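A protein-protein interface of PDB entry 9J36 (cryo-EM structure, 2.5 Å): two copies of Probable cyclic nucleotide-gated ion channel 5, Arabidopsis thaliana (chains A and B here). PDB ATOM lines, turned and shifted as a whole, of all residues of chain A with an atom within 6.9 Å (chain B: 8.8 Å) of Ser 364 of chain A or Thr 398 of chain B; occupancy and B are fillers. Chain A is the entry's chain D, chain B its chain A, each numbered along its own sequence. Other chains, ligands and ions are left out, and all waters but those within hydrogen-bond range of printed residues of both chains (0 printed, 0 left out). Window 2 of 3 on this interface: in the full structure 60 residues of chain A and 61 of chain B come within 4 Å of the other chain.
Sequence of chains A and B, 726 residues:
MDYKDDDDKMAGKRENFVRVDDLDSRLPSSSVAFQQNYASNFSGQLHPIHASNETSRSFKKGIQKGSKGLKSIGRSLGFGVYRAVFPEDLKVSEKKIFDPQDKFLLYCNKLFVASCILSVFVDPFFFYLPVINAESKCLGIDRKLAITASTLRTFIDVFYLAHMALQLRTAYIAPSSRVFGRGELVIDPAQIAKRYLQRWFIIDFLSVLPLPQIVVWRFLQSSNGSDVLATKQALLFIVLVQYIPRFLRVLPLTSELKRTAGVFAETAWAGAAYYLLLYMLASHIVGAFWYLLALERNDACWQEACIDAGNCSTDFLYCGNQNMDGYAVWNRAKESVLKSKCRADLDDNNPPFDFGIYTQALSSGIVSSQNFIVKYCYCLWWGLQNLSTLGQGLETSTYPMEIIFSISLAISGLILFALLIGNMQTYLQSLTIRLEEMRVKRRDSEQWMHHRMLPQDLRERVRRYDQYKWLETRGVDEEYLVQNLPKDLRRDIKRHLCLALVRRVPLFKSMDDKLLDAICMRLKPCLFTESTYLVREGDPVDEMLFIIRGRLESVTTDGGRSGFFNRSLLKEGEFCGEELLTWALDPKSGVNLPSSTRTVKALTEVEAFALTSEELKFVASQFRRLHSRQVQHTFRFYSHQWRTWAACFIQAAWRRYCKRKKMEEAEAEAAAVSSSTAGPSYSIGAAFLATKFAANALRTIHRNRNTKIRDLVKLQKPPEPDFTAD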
ATOM      1  N   TRP A 290      22.019 -15.128   7.867  1.00  0.00           N
ATOM      2  CA  TRP A 290      20.771 -15.827   7.610  1.00  0.00           C
ATOM      3  C   TRP A 290      19.651 -14.859   7.290  1.00  0.00           C
ATOM      4  O   TRP A 290      18.906 -15.081   6.332  1.00  0.00           O
ATOM      5  CB  TRP A 290      20.409 -16.677   8.814  1.00  0.00           C
ATOM      6  CG  TRP A 290      19.110 -17.397   8.693  1.00  0.00           C
ATOM      7  CD1 TRP A 290      18.806 -18.389   7.827  1.00  0.00           C
ATOM      8  CD2 TRP A 290      17.943 -17.181   9.481  1.00  0.00           C
ATOM      9  NE1 TRP A 290      17.524 -18.807   8.017  1.00  0.00           N
ATOM     10  CE2 TRP A 290      16.967 -18.075   9.027  1.00  0.00           C
ATOM     11  CE3 TRP A 290      17.628 -16.312  10.526  1.00  0.00           C
ATOM     12  CZ2 TRP A 290      15.705 -18.138   9.585  1.00  0.00           C
ATOM     13  CZ3 TRP A 290      16.382 -16.368  11.066  1.00  0.00           C
ATOM     14  CH2 TRP A 290      15.431 -17.276  10.603  1.00  0.00           C
ATOM     15  N   ALA A 344       5.488 -18.095   1.985  1.00  0.00           N
ATOM     16  CA  ALA A 344       6.366 -18.951   2.756  1.00  0.00           C
ATOM     17  C   ALA A 344       5.579 -19.566   3.901  1.00  0.00           C
ATOM     18  O   ALA A 344       5.104 -18.873   4.800  1.00  0.00           O
ATOM     19  CB  ALA A 344       7.574 -18.170   3.281  1.00  0.00           C
ATOM     20  N   LEU A 346       5.738 -23.231   6.545  1.00  0.00           N
ATOM     21  CA  LEU A 346       6.577 -24.344   6.977  1.00  0.00           C
ATOM     22  C   LEU A 346       5.900 -25.701   6.852  1.00  0.00           C
ATOM     23  O   LEU A 346       6.506 -26.707   7.235  1.00  0.00           O
ATOM     24  CB  LEU A 346       7.031 -24.146   8.424  1.00  0.00           C
ATOM     25  CG  LEU A 346       8.197 -23.176   8.590  1.00  0.00           C
ATOM     26  CD1 LEU A 346       8.289 -22.673  10.007  1.00  0.00           C
ATOM     27  CD2 LEU A 346       9.487 -23.850   8.181  1.00  0.00           C
ATOM     28  N   THR A 359      12.990 -20.215   4.989  1.00  0.00           N
ATOM     29  CA  THR A 359      11.543 -20.170   5.079  1.00  0.00           C
ATOM     30  C   THR A 359      11.063 -19.916   6.495  1.00  0.00           C
ATOM     31  O   THR A 359       9.951 -19.412   6.678  1.00  0.00           O
ATOM     32  CB  THR A 359      10.928 -21.459   4.530  1.00  0.00           C
ATOM     33  OG1 THR A 359       9.515 -21.443   4.744  1.00  0.00           O
ATOM     34  CG2 THR A 359      11.508 -22.655   5.195  1.00  0.00           C
ATOM     35  N   GLN A 360      11.883 -20.217   7.490  1.00  0.00           N
ATOM     36  CA  GLN A 360      11.628 -19.846   8.869  1.00  0.00           C
ATOM     37  C   GLN A 360      11.710 -18.347   9.086  1.00  0.00           C
ATOM     38  O   GLN A 360      11.033 -17.832   9.971  1.00  0.00           O
ATOM     39  CB  GLN A 360      12.619 -20.566   9.780  1.00  0.00           C
ATOM     40  CG  GLN A 360      12.225 -20.635  11.228  1.00  0.00           C
ATOM     41  CD  GLN A 360      13.378 -21.026  12.113  1.00  0.00           C
ATOM     42  OE1 GLN A 360      14.109 -21.960  11.813  1.00  0.00           O
ATOM     43  NE2 GLN A 360      13.554 -20.307  13.202  1.00  0.00           N
ATOM     44  N   ALA A 361      12.513 -17.634   8.299  1.00  0.00           N
ATOM     45  CA  ALA A 361      12.601 -16.189   8.393  1.00  0.00           C
ATOM     46  C   ALA A 361      11.428 -15.468   7.771  1.00  0.00           C
ATOM     47  O   ALA A 361      11.044 -14.412   8.266  1.00  0.00           O
ATOM     48  CB  ALA A 361      13.880 -15.681   7.725  1.00  0.00           C
ATOM     49  N   LEU A 362      10.854 -16.004   6.703  1.00  0.00           N
ATOM     50  CA  LEU A 362       9.765 -15.335   6.014  1.00  0.00           C
ATOM     51  C   LEU A 362       8.396 -15.806   6.454  1.00  0.00           C
ATOM     52  O   LEU A 362       7.430 -15.062   6.304  1.00  0.00           O
ATOM     53  CB  LEU A 362       9.906 -15.525   4.503  1.00  0.00           C
ATOM     54  CG  LEU A 362      11.333 -15.347   3.998  1.00  0.00           C
ATOM     55  CD1 LEU A 362      11.465 -16.008   2.695  1.00  0.00           C
ATOM     56  CD2 LEU A 362      11.706 -13.904   3.857  1.00  0.00           C
ATOM     57  N   SER A 363       8.290 -17.015   7.005  1.00  0.00           N
ATOM     58  CA  SER A 363       7.006 -17.477   7.509  1.00  0.00           C
ATOM     59  C   SER A 363       6.741 -16.943   8.907  1.00  0.00           C
ATOM     60  O   SER A 363       5.585 -16.733   9.287  1.00  0.00           O
ATOM     61  CB  SER A 363       6.956 -18.999   7.497  1.00  0.00           C
ATOM     62  OG  SER A 363       7.905 -19.546   8.381  1.00  0.00           O
ATOM     63  N   SER A 364       7.794 -16.716   9.689  1.00  0.00           N
ATOM     64  CA  SER A 364       7.612 -16.116  11.005  1.00  0.00           C
ATOM     65  C   SER A 364       7.329 -14.629  10.896  1.00  0.00           C
ATOM     66  O   SER A 364       6.737 -14.037  11.803  1.00  0.00           O
ATOM     67  CB  SER A 364       8.838 -16.357  11.868  1.00  0.00           C
ATOM     68  OG  SER A 364       9.874 -15.474  11.512  1.00  0.00           O
ATOM     69  N   GLY A 365       7.748 -14.009   9.804  1.00  0.00           N
ATOM     70  CA  GLY A 365       7.481 -12.610   9.580  1.00  0.00           C
ATOM     71  C   GLY A 365       8.450 -11.661  10.229  1.00  0.00           C
ATOM     72  O   GLY A 365       8.127 -10.481  10.366  1.00  0.00           O
ATOM     73  N   ILE A 366       9.628 -12.129  10.645  1.00  0.00           N
ATOM     74  CA  ILE A 366      10.626 -11.227  11.214  1.00  0.00           C
ATOM     75  C   ILE A 366      11.286 -10.347  10.172  1.00  0.00           C
ATOM     76  O   ILE A 366      11.902  -9.343  10.528  1.00  0.00           O
ATOM     77  CB  ILE A 366      11.767 -11.955  11.946  1.00  0.00           C
ATOM     78  CG1 ILE A 366      12.427 -12.941  10.992  1.00  0.00           C
ATOM     79  CG2 ILE A 366      11.262 -12.599  13.212  1.00  0.00           C
ATOM     80  CD1 ILE A 366      13.758 -13.353  11.378  1.00  0.00           C
ATOM     81  N   VAL A 367      11.174 -10.698   8.893  1.00  0.00           N
ATOM     82  CA  VAL A 367      11.715  -9.874   7.827  1.00  0.00           C
ATOM     83  C   VAL A 367      10.885  -8.627   7.613  1.00  0.00           C
ATOM     84  O   VAL A 367      11.348  -7.688   6.960  1.00  0.00           O
ATOM     85  CB  VAL A 367      11.801 -10.706   6.542  1.00  0.00           C
ATOM     86  CG1 VAL A 367      12.698 -11.888   6.771  1.00  0.00           C
ATOM     87  CG2 VAL A 367      10.433 -11.182   6.154  1.00  0.00           C
ATOM     88  N   SER A 369       9.223  -7.366  10.459  1.00  0.00           N
ATOM     89  CA  SER A 369       8.993  -7.048  11.855  1.00  0.00           C
ATOM     90  C   SER A 369       9.333  -5.591  12.108  1.00  0.00           C
ATOM     91  O   SER A 369      10.365  -5.097  11.652  1.00  0.00           O
ATOM     92  CB  SER A 369       9.839  -7.939  12.760  1.00  0.00           C
ATOM     93  OG  SER A 369       9.459  -7.807  14.109  1.00  0.00           O
ATOM     94  N   VAL A 374      12.652  -8.203  18.547  1.00  0.00           N
ATOM     95  CA  VAL A 374      12.114  -9.478  18.083  1.00  0.00           C
ATOM     96  C   VAL A 374      12.966 -10.045  16.953  1.00  0.00           C
ATOM     97  O   VAL A 374      13.357 -11.217  16.981  1.00  0.00           O
ATOM     98  CB  VAL A 374      10.650  -9.292  17.652  1.00  0.00           C
ATOM     99  CG1 VAL A 374      10.184 -10.426  16.776  1.00  0.00           C
ATOM    100  CG2 VAL A 374       9.772  -9.152  18.859  1.00  0.00           C
ATOM    101  N   LYS A 375      13.306  -9.204  15.975  1.00  0.00           N
ATOM    102  CA  LYS A 375      14.058  -9.637  14.800  1.00  0.00           C
ATOM    103  C   LYS A 375      15.476 -10.050  15.165  1.00  0.00           C
ATOM    104  O   LYS A 375      15.948 -11.116  14.752  1.00  0.00           O
ATOM    105  CB  LYS A 375      14.069  -8.510  13.769  1.00  0.00           C
ATOM    106  CG  LYS A 375      15.118  -8.628  12.688  1.00  0.00           C
ATOM    107  CD  LYS A 375      15.268  -7.338  11.918  1.00  0.00           C
ATOM    108  CE  LYS A 375      13.948  -6.894  11.353  1.00  0.00           C
ATOM    109  NZ  LYS A 375      14.097  -5.944  10.241  1.00  0.00           N
ATOM    110  N   TYR A 378      15.366 -13.295  17.380  1.00  0.00           N
ATOM    111  CA  TYR A 378      14.996 -14.445  16.576  1.00  0.00           C
ATOM    112  C   TYR A 378      16.106 -14.883  15.637  1.00  0.00           C
ATOM    113  O   TYR A 378      16.258 -16.082  15.402  1.00  0.00           O
ATOM    114  CB  TYR A 378      13.739 -14.121  15.782  1.00  0.00           C
ATOM    115  CG  TYR A 378      13.038 -15.326  15.231  1.00  0.00           C
ATOM    116  CD1 TYR A 378      13.296 -15.774  13.947  1.00  0.00           C
ATOM    117  CD2 TYR A 378      12.120 -16.019  15.992  1.00  0.00           C
ATOM    118  CE1 TYR A 378      12.657 -16.872  13.437  1.00  0.00           C
ATOM    119  CE2 TYR A 378      11.478 -17.120  15.491  1.00  0.00           C
ATOM    120  CZ  TYR A 378      11.750 -17.542  14.217  1.00  0.00           C
ATOM    121  OH  TYR A 378      11.107 -18.641  13.719  1.00  0.00           O
ATOM    122  N   ARG B 297       2.465 -18.156  29.117  1.00  0.00           N
ATOM    123  CA  ARG B 297       2.012 -17.925  27.750  1.00  0.00           C
ATOM    124  C   ARG B 297       0.555 -18.297  27.533  1.00  0.00           C
ATOM    125  O   ARG B 297      -0.137 -17.606  26.782  1.00  0.00           O
ATOM    126  CB  ARG B 297       2.876 -18.685  26.754  1.00  0.00           C
ATOM    127  CG  ARG B 297       4.225 -18.048  26.515  1.00  0.00           C
ATOM    128  CD  ARG B 297       4.160 -16.554  26.301  1.00  0.00           C
ATOM    129  NE  ARG B 297       4.043 -16.201  24.898  1.00  0.00           N
ATOM    130  CZ  ARG B 297       3.485 -15.078  24.474  1.00  0.00           C
ATOM    131  NH1 ARG B 297       3.000 -14.221  25.355  1.00  0.00           N
ATOM    132  NH2 ARG B 297       3.413 -14.811  23.181  1.00  0.00           N
ATOM    133  N   ASN B 349       0.689 -25.029  11.684  1.00  0.00           N
ATOM    134  CA  ASN B 349       1.811 -24.157  11.368  1.00  0.00           C
ATOM    135  C   ASN B 349       1.432 -22.686  11.402  1.00  0.00           C
ATOM    136  O   ASN B 349       2.320 -21.834  11.500  1.00  0.00           O
ATOM    137  CB  ASN B 349       2.403 -24.510  10.002  1.00  0.00           C
ATOM    138  CG  ASN B 349       3.352 -25.683  10.073  1.00  0.00           C
ATOM    139  OD1 ASN B 349       4.561 -25.509  10.216  1.00  0.00           O
ATOM    140  ND2 ASN B 349       2.811 -26.889   9.965  1.00  0.00           N
ATOM    141  N   ASN B 350       0.140 -22.368  11.322  1.00  0.00           N
ATOM    142  CA  ASN B 350      -0.355 -21.021  11.614  1.00  0.00           C
ATOM    143  C   ASN B 350      -1.479 -21.111  12.642  1.00  0.00           C
ATOM    144  O   ASN B 350      -2.663 -21.052  12.301  1.00  0.00           O
ATOM    145  CB  ASN B 350      -0.821 -20.318  10.341  1.00  0.00           C
ATOM    146  CG  ASN B 350      -0.438 -18.853  10.315  1.00  0.00           C
ATOM    147  OD1 ASN B 350       0.007 -18.299  11.320  1.00  0.00           O
ATOM    148  ND2 ASN B 350      -0.615 -18.215   9.165  1.00  0.00           N
ATOM    149  N   ASP B 354       0.759 -18.332  18.965  1.00  0.00           N
ATOM    150  CA  ASP B 354       1.989 -19.096  18.875  1.00  0.00           C
ATOM    151  C   ASP B 354       2.498 -19.368  20.280  1.00  0.00           C
ATOM    152  O   ASP B 354       2.813 -18.437  21.023  1.00  0.00           O
ATOM    153  CB  ASP B 354       3.035 -18.353  18.055  1.00  0.00           C
ATOM    154  CG  ASP B 354       4.003 -19.285  17.375  1.00  0.00           C
ATOM    155  OD1 ASP B 354       3.923 -20.505  17.604  1.00  0.00           O
ATOM    156  OD2 ASP B 354       4.852 -18.797  16.611  1.00  0.00           O
ATOM    157  N   PHE B 355       2.557 -20.641  20.644  1.00  0.00           N
ATOM    158  CA  PHE B 355       3.096 -21.030  21.933  1.00  0.00           C
ATOM    159  C   PHE B 355       4.550 -21.434  21.847  1.00  0.00           C
ATOM    160  O   PHE B 355       5.238 -21.432  22.864  1.00  0.00           O
ATOM    161  CB  PHE B 355       2.264 -22.165  22.522  1.00  0.00           C
ATOM    162  CG  PHE B 355       0.890 -21.746  22.918  1.00  0.00           C
ATOM    163  CD1 PHE B 355       0.700 -20.871  23.964  1.00  0.00           C
ATOM    164  CD2 PHE B 355      -0.210 -22.206  22.231  1.00  0.00           C
ATOM    165  CE1 PHE B 355      -0.559 -20.484  24.329  1.00  0.00           C
ATOM    166  CE2 PHE B 355      -1.468 -21.810  22.591  1.00  0.00           C
ATOM    167  CZ  PHE B 355      -1.639 -20.950  23.642  1.00  0.00           C
ATOM    168  N   GLY B 356       5.032 -21.768  20.666  1.00  0.00           N
ATOM    169  CA  GLY B 356       6.449 -21.923  20.466  1.00  0.00           C
ATOM    170  C   GLY B 356       7.049 -23.173  21.051  1.00  0.00           C
ATOM    171  O   GLY B 356       6.855 -24.264  20.522  1.00  0.00           O
ATOM    172  N   ILE B 357       7.812 -23.027  22.126  1.00  0.00           N
ATOM    173  CA  ILE B 357       8.436 -24.174  22.766  1.00  0.00           C
ATOM    174  C   ILE B 357       7.514 -24.691  23.855  1.00  0.00           C
ATOM    175  O   ILE B 357       7.767 -25.736  24.459  1.00  0.00           O
ATOM    176  CB  ILE B 357       9.821 -23.819  23.325  1.00  0.00           C
ATOM    177  CG1 ILE B 357       9.734 -22.679  24.322  1.00  0.00           C
ATOM    178  CG2 ILE B 357      10.729 -23.444  22.215  1.00  0.00           C
ATOM    179  CD1 ILE B 357      10.958 -22.527  25.138  1.00  0.00           C
ATOM    180  N   GLU B 395      11.349 -24.963  18.591  1.00  0.00           N
ATOM    181  CA  GLU B 395      10.779 -24.121  17.551  1.00  0.00           C
ATOM    182  C   GLU B 395      10.105 -22.960  18.256  1.00  0.00           C
ATOM    183  O   GLU B 395       8.903 -23.002  18.506  1.00  0.00           O
ATOM    184  CB  GLU B 395       9.795 -24.893  16.699  1.00  0.00           C
ATOM    185  CG  GLU B 395      10.412 -26.010  15.912  1.00  0.00           C
ATOM    186  CD  GLU B 395       9.372 -26.915  15.303  1.00  0.00           C
ATOM    187  OE1 GLU B 395       8.867 -27.803  16.020  1.00  0.00           O
ATOM    188  OE2 GLU B 395       9.055 -26.738  14.109  1.00  0.00           O
ATOM    189  N   THR B 396      10.876 -21.926  18.561  1.00  0.00           N
ATOM    190  CA  THR B 396      10.340 -20.822  19.331  1.00  0.00           C
ATOM    191  C   THR B 396       9.442 -19.950  18.475  1.00  0.00           C
ATOM    192  O   THR B 396       9.474 -19.982  17.246  1.00  0.00           O
ATOM    193  CB  THR B 396      11.450 -19.953  19.917  1.00  0.00           C
ATOM    194  OG1 THR B 396      11.930 -19.060  18.914  1.00  0.00           O
ATOM    195  CG2 THR B 396      12.578 -20.787  20.397  1.00  0.00           C
ATOM    196  N   SER B 397       8.619 -19.172  19.154  1.00  0.00           N
ATOM    197  CA  SER B 397       7.879 -18.101  18.531  1.00  0.00           C
ATOM    198  C   SER B 397       8.757 -16.855  18.491  1.00  0.00           C
ATOM    199  O   SER B 397       9.915 -16.864  18.909  1.00  0.00           O
ATOM    200  CB  SER B 397       6.577 -17.865  19.283  1.00  0.00           C
ATOM    201  OG  SER B 397       6.739 -16.907  20.298  1.00  0.00           O
ATOM    202  N   THR B 398       8.207 -15.766  17.970  1.00  0.00           N
ATOM    203  CA  THR B 398       8.924 -14.497  17.911  1.00  0.00           C
ATOM    204  C   THR B 398       8.598 -13.658  19.143  1.00  0.00           C
ATOM    205  O   THR B 398       8.111 -12.536  19.067  1.00  0.00           O
ATOM    206  CB  THR B 398       8.580 -13.757  16.627  1.00  0.00           C
ATOM    207  OG1 THR B 398       7.264 -13.214  16.734  1.00  0.00           O
ATOM    208  CG2 THR B 398       8.633 -14.688  15.448  1.00  0.00           C
ATOM    209  N   TYR B 399       8.857 -14.253  20.296  1.00  0.00           N
ATOM    210  CA  TYR B 399       8.601 -13.641  21.595  1.00  0.00           C
ATOM    211  C   TYR B 399       9.920 -13.625  22.339  1.00  0.00           C
ATOM    212  O   TYR B 399      10.508 -14.701  22.550  1.00  0.00           O
ATOM    213  CB  TYR B 399       7.539 -14.427  22.360  1.00  0.00           C
ATOM    214  CG  TYR B 399       7.249 -13.890  23.730  1.00  0.00           C
ATOM    215  CD1 TYR B 399       7.558 -14.626  24.863  1.00  0.00           C
ATOM    216  CD2 TYR B 399       6.672 -12.646  23.895  1.00  0.00           C
ATOM    217  CE1 TYR B 399       7.303 -14.138  26.117  1.00  0.00           C
ATOM    218  CE2 TYR B 399       6.414 -12.150  25.148  1.00  0.00           C
ATOM    219  CZ  TYR B 399       6.730 -12.901  26.250  1.00  0.00           C
ATOM    220  OH  TYR B 399       6.467 -12.404  27.499  1.00  0.00           O
ATOM    221  N   PRO B 400      10.437 -12.457  22.731  1.00  0.00           N
ATOM    222  CA  PRO B 400      11.855 -12.363  23.122  1.00  0.00           C
ATOM    223  C   PRO B 400      12.242 -13.062  24.414  1.00  0.00           C
ATOM    224  O   PRO B 400      13.377 -13.537  24.512  1.00  0.00           O
ATOM    225  CB  PRO B 400      12.067 -10.850  23.213  1.00  0.00           C
ATOM    226  CG  PRO B 400      11.092 -10.298  22.280  1.00  0.00           C
ATOM    227  CD  PRO B 400       9.874 -11.127  22.472  1.00  0.00           C
ATOM    228  N   MET B 401      11.354 -13.141  25.404  1.00  0.00           N
ATOM    229  CA  MET B 401      11.656 -13.881  26.622  1.00  0.00           C
ATOM    230  C   MET B 401      11.788 -15.373  26.373  1.00  0.00           C
ATOM    231  O   MET B 401      12.658 -16.017  26.963  1.00  0.00           O
ATOM    232  CB  MET B 401      10.577 -13.613  27.673  1.00  0.00           C
ATOM    233  CG  MET B 401      10.718 -14.393  28.985  1.00  0.00           C
ATOM    234  SD  MET B 401      12.226 -14.021  29.900  1.00  0.00           S
ATOM    235  CE  MET B 401      12.484 -15.544  30.811  1.00  0.00           C
ATOM    236  N   GLU B 402      10.981 -15.917  25.469  1.00  0.00           N
ATOM    237  CA  GLU B 402      11.081 -17.322  25.108  1.00  0.00           C
ATOM    238  C   GLU B 402      12.365 -17.613  24.341  1.00  0.00           C
ATOM    239  O   GLU B 402      13.005 -18.651  24.551  1.00  0.00           O
ATOM    240  CB  GLU B 402       9.851 -17.692  24.298  1.00  0.00           C
ATOM    241  CG  GLU B 402       9.968 -18.922  23.496  1.00  0.00           C
ATOM    242  CD  GLU B 402       8.705 -19.238  22.791  1.00  0.00           C
ATOM    243  OE1 GLU B 402       7.741 -18.469  22.908  1.00  0.00           O
ATOM    244  OE2 GLU B 402       8.671 -20.270  22.126  1.00  0.00           O
ATOM    245  N   ILE B 403      12.774 -16.677  23.482  1.00  0.00           N
ATOM    246  CA  ILE B 403      14.021 -16.792  22.731  1.00  0.00           C
ATOM    247  C   ILE B 403      15.211 -16.756  23.677  1.00  0.00           C
ATOM    248  O   ILE B 403      16.153 -17.543  23.549  1.00  0.00           O
ATOM    249  CB  ILE B 403      14.090 -15.675  21.673  1.00  0.00           C
ATOM    250  CG1 ILE B 403      13.259 -16.031  20.450  1.00  0.00           C
ATOM    251  CG2 ILE B 403      15.488 -15.396  21.246  1.00  0.00           C
ATOM    252  CD1 ILE B 403      12.744 -14.835  19.731  1.00  0.00           C
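Leu 362 of chain A touches none of the printed residues of chain B. No residue of chain B comes within 4 Å of Ser 363 of chain A. Gly 365 of chain A touches none of the printed residues of chain B. Printed residues of chain B within 4 Å of Tyr 378 of chain A: Thr 396, Ser 397, Thr 398 and Ile 403. Thr 398 of chain B touches just these residues of chain A: Ser 364, Val 374 and Tyr 378. Printed residues of chain A within 4 Å of Ile 403 of chain B: Tyr 378 (3.8 Å). The nearest residue of chain B that does not touch Ser 364 of chain A is Thr 396 of chain B (6.5 Å).
Of the 16 printed residues of chain A, 4 touch a printed residue of chain B. Among the printed residues, 8 pairs touch across the chains.
N of Ser 397 of chain B sits at hydrogen-bond distance from OE2 of Glu 402 of chain B, 3.2 Å away. N of Tyr 399 of chain B lies close to OG of Ser 397 of chain B, at 3.4 Å. The side-chain hydroxyl (OG) of Ser 364 of chain A sits close to the backbone NH (N) of Ile 366 of chain A. The backbone carbonyl oxygen of Gln 360 of chain A sits at hydrogen-bond distance from the side-chain hydroxyl of Ser 364 of chain A, 3.0 Å away. The side-chain hydroxyl of Tyr 378 of chain A sits at hydrogen-bond distance from the side-chain amide nitrogen of Gln 360 of chain A (3.0 Å).
Asn 349 of chain B touches Leu 346 of chain A. Thr 398 of chain B touches Ser 364 of chain A (CG2 to CB, 3.96 Å). Val 374 of chain A touches Thr 398 of chain B. CG2 of Val 374 of chain A touches CG of Pro 400 of chain B (3.8 Å). CE2 of Tyr 378 of chain A touches O of Thr 396 of chain B (3.9 Å). O of Ser 397 of chain B touches CD2 of Tyr 378 of chain A (3.8 Å). Tyr 378 of chain A touches Thr 398 of chain B. Tyr 378 of chain A touches Ile 403 of chain B (N to CD1, 3.8 Å).
No position is printed for both chains.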
